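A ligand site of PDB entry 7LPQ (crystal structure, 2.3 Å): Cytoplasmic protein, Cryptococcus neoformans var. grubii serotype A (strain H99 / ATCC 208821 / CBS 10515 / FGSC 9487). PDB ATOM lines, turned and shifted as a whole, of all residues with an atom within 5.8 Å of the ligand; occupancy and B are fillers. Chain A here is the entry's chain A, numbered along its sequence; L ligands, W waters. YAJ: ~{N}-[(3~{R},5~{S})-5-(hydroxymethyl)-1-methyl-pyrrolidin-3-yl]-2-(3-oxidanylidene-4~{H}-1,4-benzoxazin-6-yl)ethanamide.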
ATOM      1  N   LYS A  48      40.170  -5.799  -0.964  1.00  0.00           N
ATOM      2  CA  LYS A  48      38.946  -6.468  -0.544  1.00  0.00           C
ATOM      3  C   LYS A  48      38.851  -7.891  -1.057  1.00  0.00           C
ATOM      4  O   LYS A  48      38.115  -8.700  -0.474  1.00  0.00           O
ATOM      5  CB  LYS A  48      37.732  -5.680  -1.025  1.00  0.00           C
ATOM      6  CG  LYS A  48      37.389  -4.437  -0.238  1.00  0.00           C
ATOM      7  CD  LYS A  48      36.123  -3.798  -0.806  1.00  0.00           C
ATOM      8  CE  LYS A  48      35.858  -2.434  -0.191  1.00  0.00           C
ATOM      9  NZ  LYS A  48      34.683  -1.756  -0.798  1.00  0.00           N
ATOM     10  N   HIS A 143      38.298  -4.242   7.576  1.00  0.00           N
ATOM     11  CA  HIS A 143      37.280  -3.865   6.604  1.00  0.00           C
ATOM     12  C   HIS A 143      36.368  -5.043   6.250  1.00  0.00           C
ATOM     13  O   HIS A 143      36.827  -6.182   6.108  1.00  0.00           O
ATOM     14  CB  HIS A 143      37.932  -3.333   5.315  1.00  0.00           C
ATOM     15  CG  HIS A 143      37.006  -2.512   4.485  1.00  0.00           C
ATOM     16  ND1 HIS A 143      36.973  -1.138   4.551  1.00  0.00           N
ATOM     17  CD2 HIS A 143      36.049  -2.866   3.587  1.00  0.00           C
ATOM     18  CE1 HIS A 143      36.049  -0.676   3.725  1.00  0.00           C
ATOM     19  NE2 HIS A 143      35.474  -1.710   3.132  1.00  0.00           N
ATOM     20  N   ASP A 145      32.253  -5.622   4.036  1.00  0.00           N
ATOM     21  CA  ASP A 145      31.053  -5.106   3.399  1.00  0.00           C
ATOM     22  C   ASP A 145      30.033  -6.238   3.370  1.00  0.00           C
ATOM     23  O   ASP A 145      30.361  -7.344   2.908  1.00  0.00           O
ATOM     24  CB  ASP A 145      31.335  -4.606   1.978  1.00  0.00           C
ATOM     25  CG  ASP A 145      32.184  -3.370   1.959  1.00  0.00           C
ATOM     26  OD1 ASP A 145      31.650  -2.265   2.210  1.00  0.00           O
ATOM     27  OD2 ASP A 145      33.390  -3.493   1.686  1.00  0.00           O
ATOM     28  N   MET A 197      24.787   0.160  -7.200  1.00  0.00           N
ATOM     29  CA  MET A 197      24.783   0.276  -5.747  1.00  0.00           C
ATOM     30  C   MET A 197      23.695  -0.571  -5.111  1.00  0.00           C
ATOM     31  O   MET A 197      23.169  -0.242  -4.045  1.00  0.00           O
ATOM     32  CB  MET A 197      24.634   1.738  -5.328  1.00  0.00           C
ATOM     33  CG  MET A 197      25.795   2.632  -5.779  1.00  0.00           C
ATOM     34  SD  MET A 197      27.427   2.043  -5.232  1.00  0.00           S
ATOM     35  CE  MET A 197      27.250   2.267  -3.463  1.00  0.00           C
ATOM     36  N   TRP A 199      24.415  -3.627  -4.105  1.00  0.00           N
ATOM     37  CA  TRP A 199      25.098  -4.513  -3.155  1.00  0.00           C
ATOM     38  C   TRP A 199      24.813  -4.133  -1.707  1.00  0.00           C
ATOM     39  O   TRP A 199      24.756  -5.012  -0.834  1.00  0.00           O
ATOM     40  CB  TRP A 199      26.601  -4.495  -3.424  1.00  0.00           C
ATOM     41  CG  TRP A 199      27.288  -3.220  -3.055  1.00  0.00           C
ATOM     42  CD1 TRP A 199      27.622  -2.203  -3.885  1.00  0.00           C
ATOM     43  CD2 TRP A 199      27.735  -2.828  -1.750  1.00  0.00           C
ATOM     44  NE1 TRP A 199      28.245  -1.194  -3.191  1.00  0.00           N
ATOM     45  CE2 TRP A 199      28.329  -1.561  -1.873  1.00  0.00           C
ATOM     46  CE3 TRP A 199      27.703  -3.442  -0.484  1.00  0.00           C
ATOM     47  CZ2 TRP A 199      28.869  -0.886  -0.790  1.00  0.00           C
ATOM     48  CZ3 TRP A 199      28.247  -2.758   0.597  1.00  0.00           C
ATOM     49  CH2 TRP A 199      28.825  -1.490   0.434  1.00  0.00           C
ATOM     50  N   GLU A 271      31.710  -0.250   9.040  1.00  0.00           N
ATOM     51  CA  GLU A 271      30.278  -0.209   8.747  1.00  0.00           C
ATOM     52  C   GLU A 271      29.560  -1.480   9.186  1.00  0.00           C
ATOM     53  O   GLU A 271      29.020  -2.218   8.358  1.00  0.00           O
ATOM     54  CB  GLU A 271      30.072   0.031   7.235  1.00  0.00           C
ATOM     55  CG  GLU A 271      30.836   1.238   6.689  1.00  0.00           C
ATOM     56  CD  GLU A 271      30.333   1.722   5.317  1.00  0.00           C
ATOM     57  OE1 GLU A 271      29.598   0.973   4.650  1.00  0.00           O
ATOM     58  OE2 GLU A 271      30.697   2.842   4.914  1.00  0.00           O
ATOM     59  N   VAL A 431      26.685   3.033  10.440  1.00  0.00           N
ATOM     60  CA  VAL A 431      26.363   4.029   9.425  1.00  0.00           C
ATOM     61  C   VAL A 431      25.144   4.835   9.833  1.00  0.00           C
ATOM     62  O   VAL A 431      24.092   4.278  10.148  1.00  0.00           O
ATOM     63  CB  VAL A 431      26.147   3.349   8.062  1.00  0.00           C
ATOM     64  CG1 VAL A 431      25.440   4.290   7.107  1.00  0.00           C
ATOM     65  CG2 VAL A 431      27.461   2.878   7.468  1.00  0.00           C
ATOM     66  N   LEU A 432      25.299   6.163   9.833  1.00  0.00           N
ATOM     67  CA  LEU A 432      24.196   7.101  10.046  1.00  0.00           C
ATOM     68  C   LEU A 432      23.526   6.917  11.409  1.00  0.00           C
ATOM     69  O   LEU A 432      22.350   7.208  11.578  1.00  0.00           O
ATOM     70  CB  LEU A 432      23.161   6.996   8.915  1.00  0.00           C
ATOM     71  CG  LEU A 432      23.721   7.506   7.580  1.00  0.00           C
ATOM     72  CD1 LEU A 432      22.978   6.864   6.409  1.00  0.00           C
ATOM     73  CD2 LEU A 432      23.677   9.034   7.491  1.00  0.00           C
ATOM     74  N   HIS A 452      31.960   8.012   8.496  1.00  0.00           N
ATOM     75  CA  HIS A 452      32.000   8.116   7.044  1.00  0.00           C
ATOM     76  C   HIS A 452      30.906   9.072   6.567  1.00  0.00           C
ATOM     77  O   HIS A 452      29.909   9.303   7.258  1.00  0.00           O
ATOM     78  CB  HIS A 452      31.805   6.738   6.406  1.00  0.00           C
ATOM     79  CG  HIS A 452      32.831   5.732   6.812  1.00  0.00           C
ATOM     80  ND1 HIS A 452      32.817   4.419   6.366  1.00  0.00           N
ATOM     81  CD2 HIS A 452      33.892   5.824   7.647  1.00  0.00           C
ATOM     82  CE1 HIS A 452      33.821   3.763   6.909  1.00  0.00           C
ATOM     83  NE2 HIS A 452      34.486   4.591   7.692  1.00  0.00           N
ATOM     84  N   PHE A 453      31.115   9.642   5.386  1.00  0.00           N
ATOM     85  CA  PHE A 453      30.090  10.449   4.761  1.00  0.00           C
ATOM     86  C   PHE A 453      30.232  10.359   3.255  1.00  0.00           C
ATOM     87  O   PHE A 453      31.340  10.487   2.719  1.00  0.00           O
ATOM     88  CB  PHE A 453      30.133  11.920   5.173  1.00  0.00           C
ATOM     89  CG  PHE A 453      29.045  12.753   4.530  1.00  0.00           C
ATOM     90  CD1 PHE A 453      29.234  13.320   3.288  1.00  0.00           C
ATOM     91  CD2 PHE A 453      27.836  12.950   5.175  1.00  0.00           C
ATOM     92  CE1 PHE A 453      28.242  14.059   2.686  1.00  0.00           C
ATOM     93  CE2 PHE A 453      26.842  13.704   4.590  1.00  0.00           C
ATOM     94  CZ  PHE A 453      27.046  14.262   3.334  1.00  0.00           C
ATOM     95  N   TYR A 454      29.097  10.164   2.576  1.00  0.00           N
ATOM     96  CA  TYR A 454      29.036  10.213   1.122  1.00  0.00           C
ATOM     97  C   TYR A 454      27.915  11.137   0.702  1.00  0.00           C
ATOM     98  O   TYR A 454      26.915  11.268   1.394  1.00  0.00           O
ATOM     99  CB  TYR A 454      28.806   8.818   0.544  1.00  0.00           C
ATOM    100  CG  TYR A 454      30.021   7.932   0.638  1.00  0.00           C
ATOM    101  CD1 TYR A 454      31.009   7.988  -0.332  1.00  0.00           C
ATOM    102  CD2 TYR A 454      30.184   7.065   1.701  1.00  0.00           C
ATOM    103  CE1 TYR A 454      32.127   7.180  -0.242  1.00  0.00           C
ATOM    104  CE2 TYR A 454      31.287   6.266   1.805  1.00  0.00           C
ATOM    105  CZ  TYR A 454      32.267   6.325   0.831  1.00  0.00           C
ATOM    106  OH  TYR A 454      33.382   5.521   0.930  1.00  0.00           O
ATOM    107  N   ASP A 455      28.100  11.816  -0.437  1.00  0.00           N
ATOM    108  CA  ASP A 455      27.000  12.504  -1.100  1.00  0.00           C
ATOM    109  C   ASP A 455      26.062  11.438  -1.634  1.00  0.00           C
ATOM    110  O   ASP A 455      26.247  10.944  -2.754  1.00  0.00           O
ATOM    111  CB  ASP A 455      27.534  13.420  -2.196  1.00  0.00           C
ATOM    112  CG  ASP A 455      26.426  14.141  -2.939  1.00  0.00           C
ATOM    113  OD1 ASP A 455      25.224  13.963  -2.594  1.00  0.00           O
ATOM    114  OD2 ASP A 455      26.753  14.895  -3.869  1.00  0.00           O
ATOM    115  N   GLY A 456      25.064  11.062  -0.833  1.00  0.00           N
ATOM    116  CA  GLY A 456      24.302   9.859  -1.129  1.00  0.00           C
ATOM    117  C   GLY A 456      23.549   9.899  -2.451  1.00  0.00           C
ATOM    118  O   GLY A 456      23.461   8.886  -3.148  1.00  0.00           O
ATOM    119  N   LEU A 457      22.983  11.060  -2.795  1.00  0.00           N
ATOM    120  CA  LEU A 457      22.275  11.156  -4.066  1.00  0.00           C
ATOM    121  C   LEU A 457      23.224  10.935  -5.231  1.00  0.00           C
ATOM    122  O   LEU A 457      22.913  10.181  -6.167  1.00  0.00           O
ATOM    123  CB  LEU A 457      21.586  12.509  -4.184  1.00  0.00           C
ATOM    124  CG  LEU A 457      20.825  12.769  -5.485  1.00  0.00           C
ATOM    125  CD1 LEU A 457      19.646  11.805  -5.613  1.00  0.00           C
ATOM    126  CD2 LEU A 457      20.357  14.206  -5.560  1.00  0.00           C
ATOM    127  N   LEU A 459      25.996   9.312  -5.238  1.00  0.00           N
ATOM    128  CA  LEU A 459      26.558   7.968  -5.265  1.00  0.00           C
ATOM    129  C   LEU A 459      25.569   6.955  -5.823  1.00  0.00           C
ATOM    130  O   LEU A 459      25.963   6.054  -6.567  1.00  0.00           O
ATOM    131  CB  LEU A 459      27.009   7.558  -3.868  1.00  0.00           C
ATOM    132  CG  LEU A 459      27.698   6.199  -3.782  1.00  0.00           C
ATOM    133  CD1 LEU A 459      29.005   6.194  -4.583  1.00  0.00           C
ATOM    134  CD2 LEU A 459      27.955   5.833  -2.331  1.00  0.00           C
ATOM    135  N   ALA A 471      20.444  14.453   3.485  1.00  0.00           N
ATOM    136  CA  ALA A 471      20.230  13.088   3.966  1.00  0.00           C
ATOM    137  C   ALA A 471      20.118  13.054   5.481  1.00  0.00           C
ATOM    138  O   ALA A 471      19.182  12.443   6.029  1.00  0.00           O
ATOM    139  CB  ALA A 471      21.374  12.194   3.497  1.00  0.00           C
ATOM    140  N   ILE A 472      21.047  13.707   6.177  1.00  0.00           N
ATOM    141  CA  ILE A 472      21.086  13.602   7.633  1.00  0.00           C
ATOM    142  C   ILE A 472      19.878  14.299   8.260  1.00  0.00           C
ATOM    143  O   ILE A 472      19.324  13.821   9.253  1.00  0.00           O
ATOM    144  CB  ILE A 472      22.413  14.161   8.170  1.00  0.00           C
ATOM    145  CG1 ILE A 472      23.576  13.299   7.685  1.00  0.00           C
ATOM    146  CG2 ILE A 472      22.385  14.221   9.680  1.00  0.00           C
ATOM    147  CD1 ILE A 472      24.946  13.851   7.996  1.00  0.00           C
ATOM    148  N   GLU A 500      26.158  19.232   6.648  1.00  0.00           N
ATOM    149  CA  GLU A 500      26.019  17.844   7.073  1.00  0.00           C
ATOM    150  C   GLU A 500      27.291  17.359   7.755  1.00  0.00           C
ATOM    151  O   GLU A 500      27.237  16.637   8.752  1.00  0.00           O
ATOM    152  CB  GLU A 500      25.669  16.946   5.875  1.00  0.00           C
ATOM    153  CG  GLU A 500      24.293  17.247   5.267  1.00  0.00           C
ATOM    154  CD  GLU A 500      23.751  16.093   4.427  1.00  0.00           C
ATOM    155  OE1 GLU A 500      23.511  15.004   4.992  1.00  0.00           O
ATOM    156  OE2 GLU A 500      23.579  16.285   3.208  1.00  0.00           O
ATOM    157  N   GLU A 521      35.861   7.898   5.466  1.00  0.00           N
ATOM    158  CA  GLU A 521      35.531   7.626   4.079  1.00  0.00           C
ATOM    159  C   GLU A 521      34.695   8.759   3.514  1.00  0.00           C
ATOM    160  O   GLU A 521      33.721   9.179   4.136  1.00  0.00           O
ATOM    161  CB  GLU A 521      34.760   6.312   3.940  1.00  0.00           C
ATOM    162  CG  GLU A 521      35.577   5.046   4.003  1.00  0.00           C
ATOM    163  CD  GLU A 521      34.745   3.814   3.682  1.00  0.00           C
ATOM    164  OE1 GLU A 521      33.726   3.972   2.963  1.00  0.00           O
ATOM    165  OE2 GLU A 521      35.095   2.714   4.167  1.00  0.00           O
ATOM    166  N   TRP A 571      37.823   8.051  -0.226  1.00  0.00           N
ATOM    167  CA  TRP A 571      37.614   6.743  -0.827  1.00  0.00           C
ATOM    168  C   TRP A 571      37.492   6.899  -2.338  1.00  0.00           C
ATOM    169  O   TRP A 571      36.549   7.550  -2.816  1.00  0.00           O
ATOM    170  CB  TRP A 571      36.346   6.079  -0.257  1.00  0.00           C
ATOM    171  CG  TRP A 571      36.210   4.682  -0.737  1.00  0.00           C
ATOM    172  CD1 TRP A 571      35.714   4.289  -1.936  1.00  0.00           C
ATOM    173  CD2 TRP A 571      36.653   3.494  -0.070  1.00  0.00           C
ATOM    174  NE1 TRP A 571      35.826   2.922  -2.068  1.00  0.00           N
ATOM    175  CE2 TRP A 571      36.382   2.411  -0.935  1.00  0.00           C
ATOM    176  CE3 TRP A 571      37.261   3.236   1.159  1.00  0.00           C
ATOM    177  CZ2 TRP A 571      36.668   1.088  -0.594  1.00  0.00           C
ATOM    178  CZ3 TRP A 571      37.551   1.922   1.498  1.00  0.00           C
ATOM    179  CH2 TRP A 571      37.251   0.873   0.623  1.00  0.00           C
ATOM    180  N   TRP A 585      34.867  -4.065  -7.922  1.00  0.00           N
ATOM    181  CA  TRP A 585      34.096  -4.462  -6.740  1.00  0.00           C
ATOM    182  C   TRP A 585      32.680  -3.889  -6.857  1.00  0.00           C
ATOM    183  O   TRP A 585      32.462  -2.691  -6.635  1.00  0.00           O
ATOM    184  CB  TRP A 585      34.780  -3.974  -5.468  1.00  0.00           C
ATOM    185  CG  TRP A 585      34.156  -4.516  -4.221  1.00  0.00           C
ATOM    186  CD1 TRP A 585      34.383  -5.737  -3.669  1.00  0.00           C
ATOM    187  CD2 TRP A 585      33.225  -3.847  -3.361  1.00  0.00           C
ATOM    188  NE1 TRP A 585      33.641  -5.872  -2.513  1.00  0.00           N
ATOM    189  CE2 TRP A 585      32.925  -4.725  -2.313  1.00  0.00           C
ATOM    190  CE3 TRP A 585      32.622  -2.584  -3.386  1.00  0.00           C
ATOM    191  CZ2 TRP A 585      32.029  -4.388  -1.293  1.00  0.00           C
ATOM    192  CZ3 TRP A 585      31.732  -2.253  -2.385  1.00  0.00           C
ATOM    193  CH2 TRP A 585      31.450  -3.153  -1.345  1.00  0.00           C
ATOM    194  N   GLU A 588      31.441  -0.439  -8.235  1.00  0.00           N
ATOM    195  CA  GLU A 588      31.850   0.844  -7.683  1.00  0.00           C
ATOM    196  C   GLU A 588      33.066   1.361  -8.440  1.00  0.00           C
ATOM    197  O   GLU A 588      33.923   0.578  -8.852  1.00  0.00           O
ATOM    198  CB  GLU A 588      32.167   0.737  -6.202  1.00  0.00           C
ATOM    199  CG  GLU A 588      30.967   0.847  -5.292  1.00  0.00           C
ATOM    200  CD  GLU A 588      31.368   1.053  -3.837  1.00  0.00           C
ATOM    201  OE1 GLU A 588      32.585   1.187  -3.564  1.00  0.00           O
ATOM    202  OE2 GLU A 588      30.461   1.086  -2.970  1.00  0.00           O
ATOM    203  N   LEU A 590      35.315   4.619  -7.606  1.00  0.00           N
ATOM    204  CA  LEU A 590      35.655   5.818  -6.848  1.00  0.00           C
ATOM    205  C   LEU A 590      37.148   6.091  -6.810  1.00  0.00           C
ATOM    206  O   LEU A 590      37.604   6.927  -6.021  1.00  0.00           O
ATOM    207  CB  LEU A 590      35.102   5.714  -5.420  1.00  0.00           C
ATOM    208  CG  LEU A 590      33.587   5.868  -5.336  1.00  0.00           C
ATOM    209  CD1 LEU A 590      32.880   4.519  -5.442  1.00  0.00           C
ATOM    210  CD2 LEU A 590      33.181   6.565  -4.048  1.00  0.00           C
HETATM  211  C10 YAJ L   1      28.074   6.300   4.689  1.00  0.00           C
HETATM  212  C13 YAJ L   1      25.780   7.353   3.432  1.00  0.00           C
HETATM  213  C20 YAJ L   1      31.148   1.661   0.786  1.00  0.00           C
HETATM  214  C21 YAJ L   1      32.051   2.483  -0.024  1.00  0.00           C
HETATM  215  C22 YAJ L   1      33.354   1.813  -0.452  1.00  0.00           C
HETATM  216  C01 YAJ L   1      31.839   3.995  -1.868  1.00  0.00           C
HETATM  217  C03 YAJ L   1      29.973   3.309  -0.544  1.00  0.00           C
HETATM  218  C04 YAJ L   1      29.742   2.324   0.697  1.00  0.00           C
HETATM  219  C06 YAJ L   1      28.121   3.408   2.317  1.00  0.00           C
HETATM  220  C08 YAJ L   1      27.681   3.928   3.710  1.00  0.00           C
HETATM  221  C09 YAJ L   1      27.309   5.418   3.903  1.00  0.00           C
HETATM  222  C11 YAJ L   1      27.719   7.653   4.857  1.00  0.00           C
HETATM  223  C12 YAJ L   1      26.576   8.212   4.235  1.00  0.00           C
HETATM  224  C14 YAJ L   1      26.166   5.989   3.288  1.00  0.00           C
HETATM  225  C16 YAJ L   1      24.276   9.247   2.873  1.00  0.00           C
HETATM  226  C18 YAJ L   1      25.226  10.159   3.509  1.00  0.00           C
HETATM  227  N02 YAJ L   1      31.184   2.828  -1.201  1.00  0.00           N
HETATM  228  N05 YAJ L   1      29.313   2.856   2.000  1.00  0.00           N
HETATM  229  N15 YAJ L   1      24.603   7.916   2.809  1.00  0.00           N
HETATM  230  O07 YAJ L   1      27.290   3.484   1.400  1.00  0.00           O
HETATM  231  O17 YAJ L   1      23.272   9.697   2.312  1.00  0.00           O
HETATM  232  O19 YAJ L   1      26.224   9.520   4.409  1.00  0.00           O
HETATM  233  O23 YAJ L   1      33.091   0.561  -1.067  1.00  0.00           O
HETATM  234  O   HOH W   1      33.084   1.193   3.617  1.00  0.00           O
HETATM  235  O   HOH W   2      24.344  12.249   1.700  1.00  0.00           O
HETATM  236  O   HOH W   3      33.644  -0.394   1.637  1.00  0.00           O
HETATM  237  O   HOH W   4      25.012   1.753   0.394  1.00  0.00           O
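A ring nitrogen (ND1) of His 452 sits at hydrogen-bond distance from the side-chain carboxylate of Glu 271. The side-chain carboxylate (OD2) of Asp 145 is in salt-bridge range of the side-chain amino group (NZ) of Lys 48 (3.3 Å). The indole nitrogen (NE1) of Trp 199 sits at hydrogen-bond distance from the side-chain carboxylate (OE2) of Glu 588, 3.2 Å away. OH of Tyr 454 is in hydrogen-bond range of OE1 of Glu 521 (2.6 Å). N of Ala 471 sits at hydrogen-bond distance from OE1 of Glu 500. N of Phe 453 sits at hydrogen-bond distance from O of Glu 521 (2.9 Å).
An oxygen (O23) of the ligand lies within hydrogen-bond range of the side-chain amino group (NZ) of Lys 48 (2.8 Å). The side-chain carboxylate (OE2) of Glu 271 lies within hydrogen-bond range of a nitrogen (N05) of the ligand, 3.2 Å away. N02 of the ligand lies within salt-bridge range of OE2 of Glu 588, 2.6 Å away. N of Tyr 454 lies within hydrogen-bond range of O19 of the ligand (3.5 Å).
Water W2 lies within hydrogen-bond range of the backbone carbonyl oxygen of Tyr 454 (2.8 Å), an oxygen (O17) of the ligand (2.8 Å) and the backbone NH of Gly 456 (2.9 Å). Water W3 lies within hydrogen-bond range of a ring nitrogen (NE2) of His 143 (2.7 Å), the side-chain carboxylate (OD1) of Asp 145 (2.8 Å), an oxygen (O23) of the ligand (2.9 Å) and the side-chain amino group (NZ) of Lys 48 (3.0 Å). Water W1 lies within hydrogen-bond range of OE2 of Glu 521 (2.6 Å) and OE2 of Glu 271 (3.2 Å).
Trp 199 touches the ligand (CZ2 to C04, 3.6 Å). Val 431 touches the ligand (CG1 to C09, 3.9 Å). His 452 touches the ligand (O to C11, 3.6 Å). CA of Phe 453 touches C11 of the ligand, at 3.7 Å. Gly 456 touches the ligand (CA to O17, 3.6 Å). CD2 of Leu 459 touches C03 of the ligand (3.7 Å). CB of Ala 471 touches O17 of the ligand, 3.4 Å away. Glu 521 touches the ligand (OE1 to C21, 3.7 Å). CE2 of Trp 571 touches C22 of the ligand, at 3.1 Å. Trp 585 touches the ligand (CZ3 to O23, 3.4 Å). Leu 590 touches the ligand. Hydrophobic or aromatic side chains within 4 Å of the ligand: Trp 199, Val 431, Phe 453, Tyr 454, Leu 459, Ala 471, Trp 571, Trp 585 and Leu 590. Of the 23 residues printed, 15 come within 4 Å of the ligand. The nearest printed residue that does not touch the ligand is Leu 432 (4.03 Å).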
